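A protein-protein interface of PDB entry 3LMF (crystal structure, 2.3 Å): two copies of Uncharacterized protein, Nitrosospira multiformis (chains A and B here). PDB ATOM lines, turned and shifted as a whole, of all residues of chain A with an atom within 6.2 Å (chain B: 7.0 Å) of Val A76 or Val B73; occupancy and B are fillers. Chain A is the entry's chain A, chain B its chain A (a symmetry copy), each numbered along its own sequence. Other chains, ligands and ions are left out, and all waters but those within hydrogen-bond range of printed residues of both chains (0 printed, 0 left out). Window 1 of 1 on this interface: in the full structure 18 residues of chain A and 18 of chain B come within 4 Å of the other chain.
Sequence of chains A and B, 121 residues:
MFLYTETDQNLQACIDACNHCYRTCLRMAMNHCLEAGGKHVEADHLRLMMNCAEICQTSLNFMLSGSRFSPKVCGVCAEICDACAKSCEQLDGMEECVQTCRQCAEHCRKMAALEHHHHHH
Lys A72 touches Val B76, and with the chains exchanged Val A76 touches Lys B72. Val A73 touches Val B76, and with the chains exchanged Val A76 touches Val B73. Val B76 touches its own counterpart, Val A76. Of the 8 pairs that touch across the chains among the printed residues, 5 have their exchanged pair printed and touching as well.
Printed residues of chain A that touch a printed residue of chain B: Lys A72, Val A73, Val A76, Glu A79 and Ile A80. Of the 19 printed residues of chain B, 5 touch a printed residue of chain A. Among the printed residues, 8 pairs touch across the chains. Among the printed residues, Asp or Glu carboxylates within 4 Å of a Lys or Arg side-chain nitrogen of the other chain: Glu A79 with Lys B72 (2.5 Å).
The backbone NH (N) of Ser B67 sits at hydrogen-bond distance from the backbone carbonyl oxygen (O) of Phe B62 (2.9 Å). The backbone carbonyl oxygen (O) of Phe B62 lies close to the side-chain hydroxyl (OG) of Ser B70 (3.4 Å). The side-chain hydroxyl (OG) of Ser B67 sits at hydrogen-bond distance from the backbone NH (N) of Phe B69 (2.9 Å).
Of the printed residues of chain B, Lys A72 touches Val B76 (3.6 Å). Val A76 touches just these residues of chain B: Lys B72 (3.6 Å), Val B73 (3.96 Å) and Val B76 (3.4 Å). Of the printed residues of chain B, Glu A79 touches Lys B72 (2.5 Å). Of the printed residues of chain A, Phe B62 touches Ile A80 (3.6 Å). Of the printed residues of chain A, Phe B69 touches Ile A80. Of chain A, only Val A76 (3.96 Å) comes within 4 Å of Val B73. Cys B74 touches none of the printed residues of chain A. Of the printed residues of chain A, Val B76 touches Lys A72, Val A73 and Val A76. Cys B77 touches none of the printed residues of chain A. The nearest printed residue of chain A that does not touch Phe B69 is Glu A79 (4.02 Å).
OE1 of Glu A79 lies within salt-bridge range of NZ of Lys B72 (2.5 Å).
Val B76 touches Lys A72 (CG2 to CG, 3.6 Å). Val B76 touches Val A73. CG2 of Val A76 touches CG of Lys B72 (3.6 Å). Val B73 touches Val A76. Val B76 touches Val A76 (CG2 to CG2, 3.4 Å). Phe B62 touches Ile A80 (CE2 to CD1, 3.6 Å). Ile A80 touches Phe B69.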
ATOM      1  N   ILE A  55       3.885 -15.211  32.667  1.00  0.00           N
ATOM      2  CA  ILE A  55       4.405 -14.190  31.770  1.00  0.00           C
ATOM      3  C   ILE A  55       4.482 -12.818  32.450  1.00  0.00           C
ATOM      4  O   ILE A  55       5.464 -12.102  32.267  1.00  0.00           O
ATOM      5  CB  ILE A  55       3.574 -14.095  30.449  1.00  0.00           C
ATOM      6  CG1 ILE A  55       4.345 -13.281  29.399  1.00  0.00           C
ATOM      7  CG2 ILE A  55       2.252 -13.399  30.701  1.00  0.00           C
ATOM      8  CD1 ILE A  55       5.735 -13.823  29.062  1.00  0.00           C
ATOM      9  N   PRO A  71      10.867  -4.757  26.201  1.00  0.00           N
ATOM     10  CA  PRO A  71       9.843  -4.472  25.189  1.00  0.00           C
ATOM     11  C   PRO A  71       9.301  -5.731  24.519  1.00  0.00           C
ATOM     12  O   PRO A  71       8.091  -5.912  24.414  1.00  0.00           O
ATOM     13  CB  PRO A  71      10.580  -3.564  24.203  1.00  0.00           C
ATOM     14  CG  PRO A  71      11.495  -2.788  25.113  1.00  0.00           C
ATOM     15  CD  PRO A  71      12.049  -3.900  25.997  1.00  0.00           C
ATOM     16  N   LYS A  72      10.209  -6.595  24.078  1.00  0.00           N
ATOM     17  CA  LYS A  72       9.841  -7.839  23.413  1.00  0.00           C
ATOM     18  C   LYS A  72       8.993  -8.725  24.343  1.00  0.00           C
ATOM     19  O   LYS A  72       7.920  -9.203  23.962  1.00  0.00           O
ATOM     20  CB  LYS A  72      11.113  -8.584  22.989  1.00  0.00           C
ATOM     21  CG  LYS A  72      10.899  -9.693  21.961  1.00  0.00           C
ATOM     22  CD  LYS A  72      10.608  -9.132  20.569  1.00  0.00           C
ATOM     23  CE  LYS A  72      10.147 -10.227  19.607  1.00  0.00           C
ATOM     24  NZ  LYS A  72      11.137 -11.349  19.441  1.00  0.00           N
ATOM     25  N   VAL A  73       9.478  -8.938  25.561  1.00  0.00           N
ATOM     26  CA  VAL A  73       8.764  -9.750  26.537  1.00  0.00           C
ATOM     27  C   VAL A  73       7.392  -9.168  26.841  1.00  0.00           C
ATOM     28  O   VAL A  73       6.404  -9.898  26.949  1.00  0.00           O
ATOM     29  CB  VAL A  73       9.559  -9.856  27.849  1.00  0.00           C
ATOM     30  CG1 VAL A  73       8.703 -10.492  28.933  1.00  0.00           C
ATOM     31  CG2 VAL A  73      10.818 -10.677  27.612  1.00  0.00           C
ATOM     32  N   CYS A  74       7.334  -7.851  26.982  1.00  0.00           N
ATOM     33  CA  CYS A  74       6.072  -7.183  27.277  1.00  0.00           C
ATOM     34  C   CYS A  74       5.057  -7.354  26.149  1.00  0.00           C
ATOM     35  O   CYS A  74       3.865  -7.497  26.408  1.00  0.00           O
ATOM     36  CB  CYS A  74       6.306  -5.694  27.544  1.00  0.00           C
ATOM     37  SG  CYS A  74       7.000  -5.331  29.164  1.00  0.00           S
ATOM     38  N   GLY A  75       5.533  -7.347  24.906  1.00  0.00           N
ATOM     39  CA  GLY A  75       4.640  -7.518  23.772  1.00  0.00           C
ATOM     40  C   GLY A  75       3.916  -8.853  23.848  1.00  0.00           C
ATOM     41  O   GLY A  75       2.726  -8.956  23.539  1.00  0.00           O
ATOM     42  N   VAL A  76       4.641  -9.884  24.263  1.00  0.00           N
ATOM     43  CA  VAL A  76       4.065 -11.210  24.388  1.00  0.00           C
ATOM     44  C   VAL A  76       3.136 -11.229  25.594  1.00  0.00           C
ATOM     45  O   VAL A  76       2.060 -11.835  25.554  1.00  0.00           O
ATOM     46  CB  VAL A  76       5.163 -12.266  24.562  1.00  0.00           C
ATOM     47  CG1 VAL A  76       4.556 -13.616  24.891  1.00  0.00           C
ATOM     48  CG2 VAL A  76       5.986 -12.351  23.283  1.00  0.00           C
ATOM     49  N   CYS A  77       3.544 -10.548  26.660  1.00  0.00           N
ATOM     50  CA  CYS A  77       2.736 -10.487  27.865  1.00  0.00           C
ATOM     51  C   CYS A  77       1.383  -9.832  27.589  1.00  0.00           C
ATOM     52  O   CYS A  77       0.363 -10.281  28.103  1.00  0.00           O
ATOM     53  CB  CYS A  77       3.487  -9.726  28.964  1.00  0.00           C
ATOM     54  SG  CYS A  77       2.697  -9.749  30.600  1.00  0.00           S
ATOM     55  N   ALA A  78       1.368  -8.777  26.776  1.00  0.00           N
ATOM     56  CA  ALA A  78       0.110  -8.090  26.461  1.00  0.00           C
ATOM     57  C   ALA A  78      -0.863  -9.024  25.750  1.00  0.00           C
ATOM     58  O   ALA A  78      -2.061  -9.016  26.027  1.00  0.00           O
ATOM     59  CB  ALA A  78       0.375  -6.868  25.590  1.00  0.00           C
ATOM     60  N   GLU A  79      -0.337  -9.835  24.840  1.00  0.00           N
ATOM     61  CA  GLU A  79      -1.158 -10.767  24.088  1.00  0.00           C
ATOM     62  C   GLU A  79      -1.821 -11.791  25.017  1.00  0.00           C
ATOM     63  O   GLU A  79      -3.015 -12.060  24.898  1.00  0.00           O
ATOM     64  CB  GLU A  79      -0.297 -11.472  23.044  1.00  0.00           C
ATOM     65  CG  GLU A  79      -1.073 -12.095  21.912  1.00  0.00           C
ATOM     66  CD  GLU A  79      -0.161 -12.596  20.805  1.00  0.00           C
ATOM     67  OE1 GLU A  79       0.687 -11.806  20.337  1.00  0.00           O
ATOM     68  OE2 GLU A  79      -0.292 -13.772  20.407  1.00  0.00           O
ATOM     69  N   ILE A  80      -1.047 -12.344  25.947  1.00  0.00           N
ATOM     70  CA  ILE A  80      -1.563 -13.334  26.889  1.00  0.00           C
ATOM     71  C   ILE A  80      -2.559 -12.716  27.869  1.00  0.00           C
ATOM     72  O   ILE A  80      -3.545 -13.346  28.237  1.00  0.00           O
ATOM     73  CB  ILE A  80      -0.400 -14.005  27.660  1.00  0.00           C
ATOM     74  CG1 ILE A  80       0.495 -14.741  26.669  1.00  0.00           C
ATOM     75  CG2 ILE A  80      -0.935 -14.955  28.719  1.00  0.00           C
ATOM     76  CD1 ILE A  80       1.816 -15.207  27.243  1.00  0.00           C
ATOM     77  N   CYS A  81      -2.302 -11.480  28.282  1.00  0.00           N
ATOM     78  CA  CYS A  81      -3.200 -10.785  29.197  1.00  0.00           C
ATOM     79  C   CYS A  81      -4.567 -10.554  28.544  1.00  0.00           C
ATOM     80  O   CYS A  81      -5.600 -10.739  29.189  1.00  0.00           O
ATOM     81  CB  CYS A  81      -2.600  -9.441  29.632  1.00  0.00           C
ATOM     82  SG  CYS A  81      -1.215  -9.565  30.829  1.00  0.00           S
ATOM     83  N   ALA A 112       6.203  -2.413  24.682  1.00  0.00           N
ATOM     84  CA  ALA A 112       6.583  -3.082  23.446  1.00  0.00           C
ATOM     85  C   ALA A 112       6.772  -2.086  22.304  1.00  0.00           C
ATOM     86  O   ALA A 112       7.620  -2.282  21.438  1.00  0.00           O
ATOM     87  CB  ALA A 112       5.526  -4.117  23.064  1.00  0.00           C
ATOM     88  N   ILE B  55      13.997 -16.316  30.744  1.00  0.00           N
ATOM     89  CA  ILE B  55      13.167 -16.584  29.579  1.00  0.00           C
ATOM     90  C   ILE B  55      13.140 -18.077  29.229  1.00  0.00           C
ATOM     91  O   ILE B  55      12.081 -18.606  28.900  1.00  0.00           O
ATOM     92  CB  ILE B  55      13.613 -15.746  28.337  1.00  0.00           C
ATOM     93  CG1 ILE B  55      12.522 -15.782  27.258  1.00  0.00           C
ATOM     94  CG2 ILE B  55      14.883 -16.315  27.739  1.00  0.00           C
ATOM     95  CD1 ILE B  55      11.150 -15.284  27.715  1.00  0.00           C
ATOM     96  N   CYS B  56      14.273 -18.772  29.327  1.00  0.00           N
ATOM     97  CA  CYS B  56      14.277 -20.202  29.010  1.00  0.00           C
ATOM     98  C   CYS B  56      13.388 -20.965  29.988  1.00  0.00           C
ATOM     99  O   CYS B  56      12.666 -21.885  29.600  1.00  0.00           O
ATOM    100  CB  CYS B  56      15.696 -20.772  29.051  1.00  0.00           C
ATOM    101  SG  CYS B  56      16.732 -20.246  27.671  1.00  0.00           S
ATOM    102  N   THR B  58      10.829 -19.781  31.495  1.00  0.00           N
ATOM    103  CA  THR B  58       9.449 -19.427  31.185  1.00  0.00           C
ATOM    104  C   THR B  58       8.960 -20.268  30.002  1.00  0.00           C
ATOM    105  O   THR B  58       7.869 -20.838  30.037  1.00  0.00           O
ATOM    106  CB  THR B  58       9.338 -17.911  30.870  1.00  0.00           C
ATOM    107  OG1 THR B  58       9.719 -17.165  32.033  1.00  0.00           O
ATOM    108  CG2 THR B  58       7.918 -17.530  30.473  1.00  0.00           C
ATOM    109  N   SER B  59       9.781 -20.356  28.965  1.00  0.00           N
ATOM    110  CA  SER B  59       9.438 -21.153  27.786  1.00  0.00           C
ATOM    111  C   SER B  59       9.217 -22.602  28.208  1.00  0.00           C
ATOM    112  O   SER B  59       8.248 -23.239  27.803  1.00  0.00           O
ATOM    113  CB  SER B  59      10.568 -21.076  26.761  1.00  0.00           C
ATOM    114  OG  SER B  59      10.698 -19.742  26.277  1.00  0.00           O
ATOM    115  N   LEU B  60      10.126 -23.112  29.031  1.00  0.00           N
ATOM    116  CA  LEU B  60      10.021 -24.473  29.533  1.00  0.00           C
ATOM    117  C   LEU B  60       8.683 -24.659  30.239  1.00  0.00           C
ATOM    118  O   LEU B  60       7.975 -25.625  29.993  1.00  0.00           O
ATOM    119  CB  LEU B  60      11.165 -24.765  30.513  1.00  0.00           C
ATOM    120  CG  LEU B  60      11.103 -26.103  31.261  1.00  0.00           C
ATOM    121  CD1 LEU B  60      11.102 -27.253  30.263  1.00  0.00           C
ATOM    122  CD2 LEU B  60      12.291 -26.216  32.205  1.00  0.00           C
ATOM    123  N   PHE B  62       5.896 -22.874  29.932  1.00  0.00           N
ATOM    124  CA  PHE B  62       4.769 -22.765  29.019  1.00  0.00           C
ATOM    125  C   PHE B  62       4.528 -24.060  28.254  1.00  0.00           C
ATOM    126  O   PHE B  62       3.392 -24.495  28.105  1.00  0.00           O
ATOM    127  CB  PHE B  62       4.977 -21.598  28.040  1.00  0.00           C
ATOM    128  CG  PHE B  62       4.342 -20.319  28.491  1.00  0.00           C
ATOM    129  CD1 PHE B  62       4.699 -19.741  29.708  1.00  0.00           C
ATOM    130  CD2 PHE B  62       3.363 -19.704  27.717  1.00  0.00           C
ATOM    131  CE1 PHE B  62       4.088 -18.565  30.151  1.00  0.00           C
ATOM    132  CE2 PHE B  62       2.748 -18.529  28.152  1.00  0.00           C
ATOM    133  CZ  PHE B  62       3.109 -17.959  29.369  1.00  0.00           C
ATOM    134  N   SER B  67       0.680 -24.784  27.072  1.00  0.00           N
ATOM    135  CA  SER B  67       0.144 -23.483  26.679  1.00  0.00           C
ATOM    136  C   SER B  67       0.035 -23.352  25.172  1.00  0.00           C
ATOM    137  O   SER B  67       0.845 -23.907  24.429  1.00  0.00           O
ATOM    138  CB  SER B  67       1.037 -22.358  27.195  1.00  0.00           C
ATOM    139  OG  SER B  67       0.606 -21.094  26.703  1.00  0.00           O
ATOM    140  N   PHE B  69       0.347 -20.572  23.867  1.00  0.00           N
ATOM    141  CA  PHE B  69       1.175 -19.409  23.596  1.00  0.00           C
ATOM    142  C   PHE B  69       2.679 -19.713  23.578  1.00  0.00           C
ATOM    143  O   PHE B  69       3.492 -18.803  23.466  1.00  0.00           O
ATOM    144  CB  PHE B  69       0.880 -18.290  24.603  1.00  0.00           C
ATOM    145  CG  PHE B  69      -0.471 -17.652  24.425  1.00  0.00           C
ATOM    146  CD1 PHE B  69      -1.567 -18.084  25.166  1.00  0.00           C
ATOM    147  CD2 PHE B  69      -0.659 -16.648  23.479  1.00  0.00           C
ATOM    148  CE1 PHE B  69      -2.832 -17.523  24.965  1.00  0.00           C
ATOM    149  CE2 PHE B  69      -1.923 -16.079  23.268  1.00  0.00           C
ATOM    150  CZ  PHE B  69      -3.010 -16.519  24.012  1.00  0.00           C
ATOM    151  N   SER B  70       3.048 -20.987  23.675  1.00  0.00           N
ATOM    152  CA  SER B  70       4.458 -21.368  23.657  1.00  0.00           C
ATOM    153  C   SER B  70       5.202 -20.823  22.436  1.00  0.00           C
ATOM    154  O   SER B  70       6.304 -20.300  22.560  1.00  0.00           O
ATOM    155  CB  SER B  70       4.619 -22.893  23.694  1.00  0.00           C
ATOM    156  OG  SER B  70       4.158 -23.431  24.920  1.00  0.00           O
ATOM    157  N   PRO B  71       4.614 -20.944  21.238  1.00  0.00           N
ATOM    158  CA  PRO B  71       5.307 -20.428  20.052  1.00  0.00           C
ATOM    159  C   PRO B  71       5.774 -18.985  20.216  1.00  0.00           C
ATOM    160  O   PRO B  71       6.926 -18.664  19.938  1.00  0.00           O
ATOM    161  CB  PRO B  71       4.257 -20.575  18.951  1.00  0.00           C
ATOM    162  CG  PRO B  71       3.540 -21.833  19.363  1.00  0.00           C
ATOM    163  CD  PRO B  71       3.343 -21.587  20.855  1.00  0.00           C
ATOM    164  N   LYS B  72       4.868 -18.127  20.675  1.00  0.00           N
ATOM    165  CA  LYS B  72       5.167 -16.715  20.878  1.00  0.00           C
ATOM    166  C   LYS B  72       6.308 -16.539  21.897  1.00  0.00           C
ATOM    167  O   LYS B  72       7.285 -15.829  21.640  1.00  0.00           O
ATOM    168  CB  LYS B  72       3.905 -15.995  21.370  1.00  0.00           C
ATOM    169  CG  LYS B  72       3.948 -14.472  21.264  1.00  0.00           C
ATOM    170  CD  LYS B  72       3.812 -13.998  19.816  1.00  0.00           C
ATOM    171  CE  LYS B  72       4.109 -12.504  19.685  1.00  0.00           C
ATOM    172  NZ  LYS B  72       3.220 -11.628  20.529  1.00  0.00           N
ATOM    173  N   VAL B  73       6.179 -17.191  23.048  1.00  0.00           N
ATOM    174  CA  VAL B  73       7.196 -17.114  24.087  1.00  0.00           C
ATOM    175  C   VAL B  73       8.538 -17.623  23.585  1.00  0.00           C
ATOM    176  O   VAL B  73       9.584 -17.035  23.868  1.00  0.00           O
ATOM    177  CB  VAL B  73       6.783 -17.935  25.320  1.00  0.00           C
ATOM    178  CG1 VAL B  73       7.948 -18.049  26.291  1.00  0.00           C
ATOM    179  CG2 VAL B  73       5.590 -17.274  25.993  1.00  0.00           C
ATOM    180  N   CYS B  74       8.506 -18.721  22.842  1.00  0.00           N
ATOM    181  CA  CYS B  74       9.731 -19.300  22.307  1.00  0.00           C
ATOM    182  C   CYS B  74      10.429 -18.361  21.327  1.00  0.00           C
ATOM    183  O   CYS B  74      11.656 -18.301  21.296  1.00  0.00           O
ATOM    184  CB  CYS B  74       9.435 -20.637  21.623  1.00  0.00           C
ATOM    185  SG  CYS B  74       9.155 -22.006  22.758  1.00  0.00           S
ATOM    186  N   GLY B  75       9.647 -17.627  20.538  1.00  0.00           N
ATOM    187  CA  GLY B  75      10.227 -16.696  19.585  1.00  0.00           C
ATOM    188  C   GLY B  75      11.070 -15.647  20.294  1.00  0.00           C
ATOM    189  O   GLY B  75      12.142 -15.259  19.824  1.00  0.00           O
ATOM    190  N   VAL B  76      10.579 -15.184  21.437  1.00  0.00           N
ATOM    191  CA  VAL B  76      11.290 -14.188  22.216  1.00  0.00           C
ATOM    192  C   VAL B  76      12.498 -14.846  22.867  1.00  0.00           C
ATOM    193  O   VAL B  76      13.580 -14.252  22.941  1.00  0.00           O
ATOM    194  CB  VAL B  76      10.380 -13.588  23.296  1.00  0.00           C
ATOM    195  CG1 VAL B  76      11.178 -12.700  24.230  1.00  0.00           C
ATOM    196  CG2 VAL B  76       9.266 -12.794  22.628  1.00  0.00           C
ATOM    197  N   CYS B  77      12.320 -16.081  23.322  1.00  0.00           N
ATOM    198  CA  CYS B  77      13.404 -16.813  23.955  1.00  0.00           C
ATOM    199  C   CYS B  77      14.569 -17.014  22.986  1.00  0.00           C
ATOM    200  O   CYS B  77      15.725 -16.896  23.380  1.00  0.00           O
ATOM    201  CB  CYS B  77      12.895 -18.163  24.472  1.00  0.00           C
ATOM    202  SG  CYS B  77      14.082 -19.103  25.477  1.00  0.00           S
ATOM    203  N   ALA B  78      14.273 -17.312  21.723  1.00  0.00           N
ATOM    204  CA  ALA B  78      15.334 -17.522  20.732  1.00  0.00           C
ATOM    205  C   ALA B  78      16.172 -16.262  20.549  1.00  0.00           C
ATOM    206  O   ALA B  78      17.395 -16.329  20.435  1.00  0.00           O
ATOM    207  CB  ALA B  78      14.737 -17.938  19.394  1.00  0.00           C
ATOM    208  N   CYS B 108      13.825 -23.148  19.693  1.00  0.00           N
ATOM    209  CA  CYS B 108      12.802 -22.165  19.977  1.00  0.00           C
ATOM    210  C   CYS B 108      12.292 -21.542  18.683  1.00  0.00           C
ATOM    211  O   CYS B 108      11.095 -21.277  18.557  1.00  0.00           O
ATOM    212  CB  CYS B 108      13.335 -21.101  20.938  1.00  0.00           C
ATOM    213  SG  CYS B 108      13.407 -21.687  22.669  1.00  0.00           S
ATOM    214  N   ALA B 112       8.477 -21.347  17.435  1.00  0.00           N
ATOM    215  CA  ALA B 112       7.854 -20.088  17.053  1.00  0.00           C
ATOM    216  C   ALA B 112       7.281 -20.153  15.638  1.00  0.00           C
ATOM    217  O   ALA B 112       6.259 -19.535  15.350  1.00  0.00           O
ATOM    218  CB  ALA B 112       8.869 -18.950  17.152  1.00  0.00           C
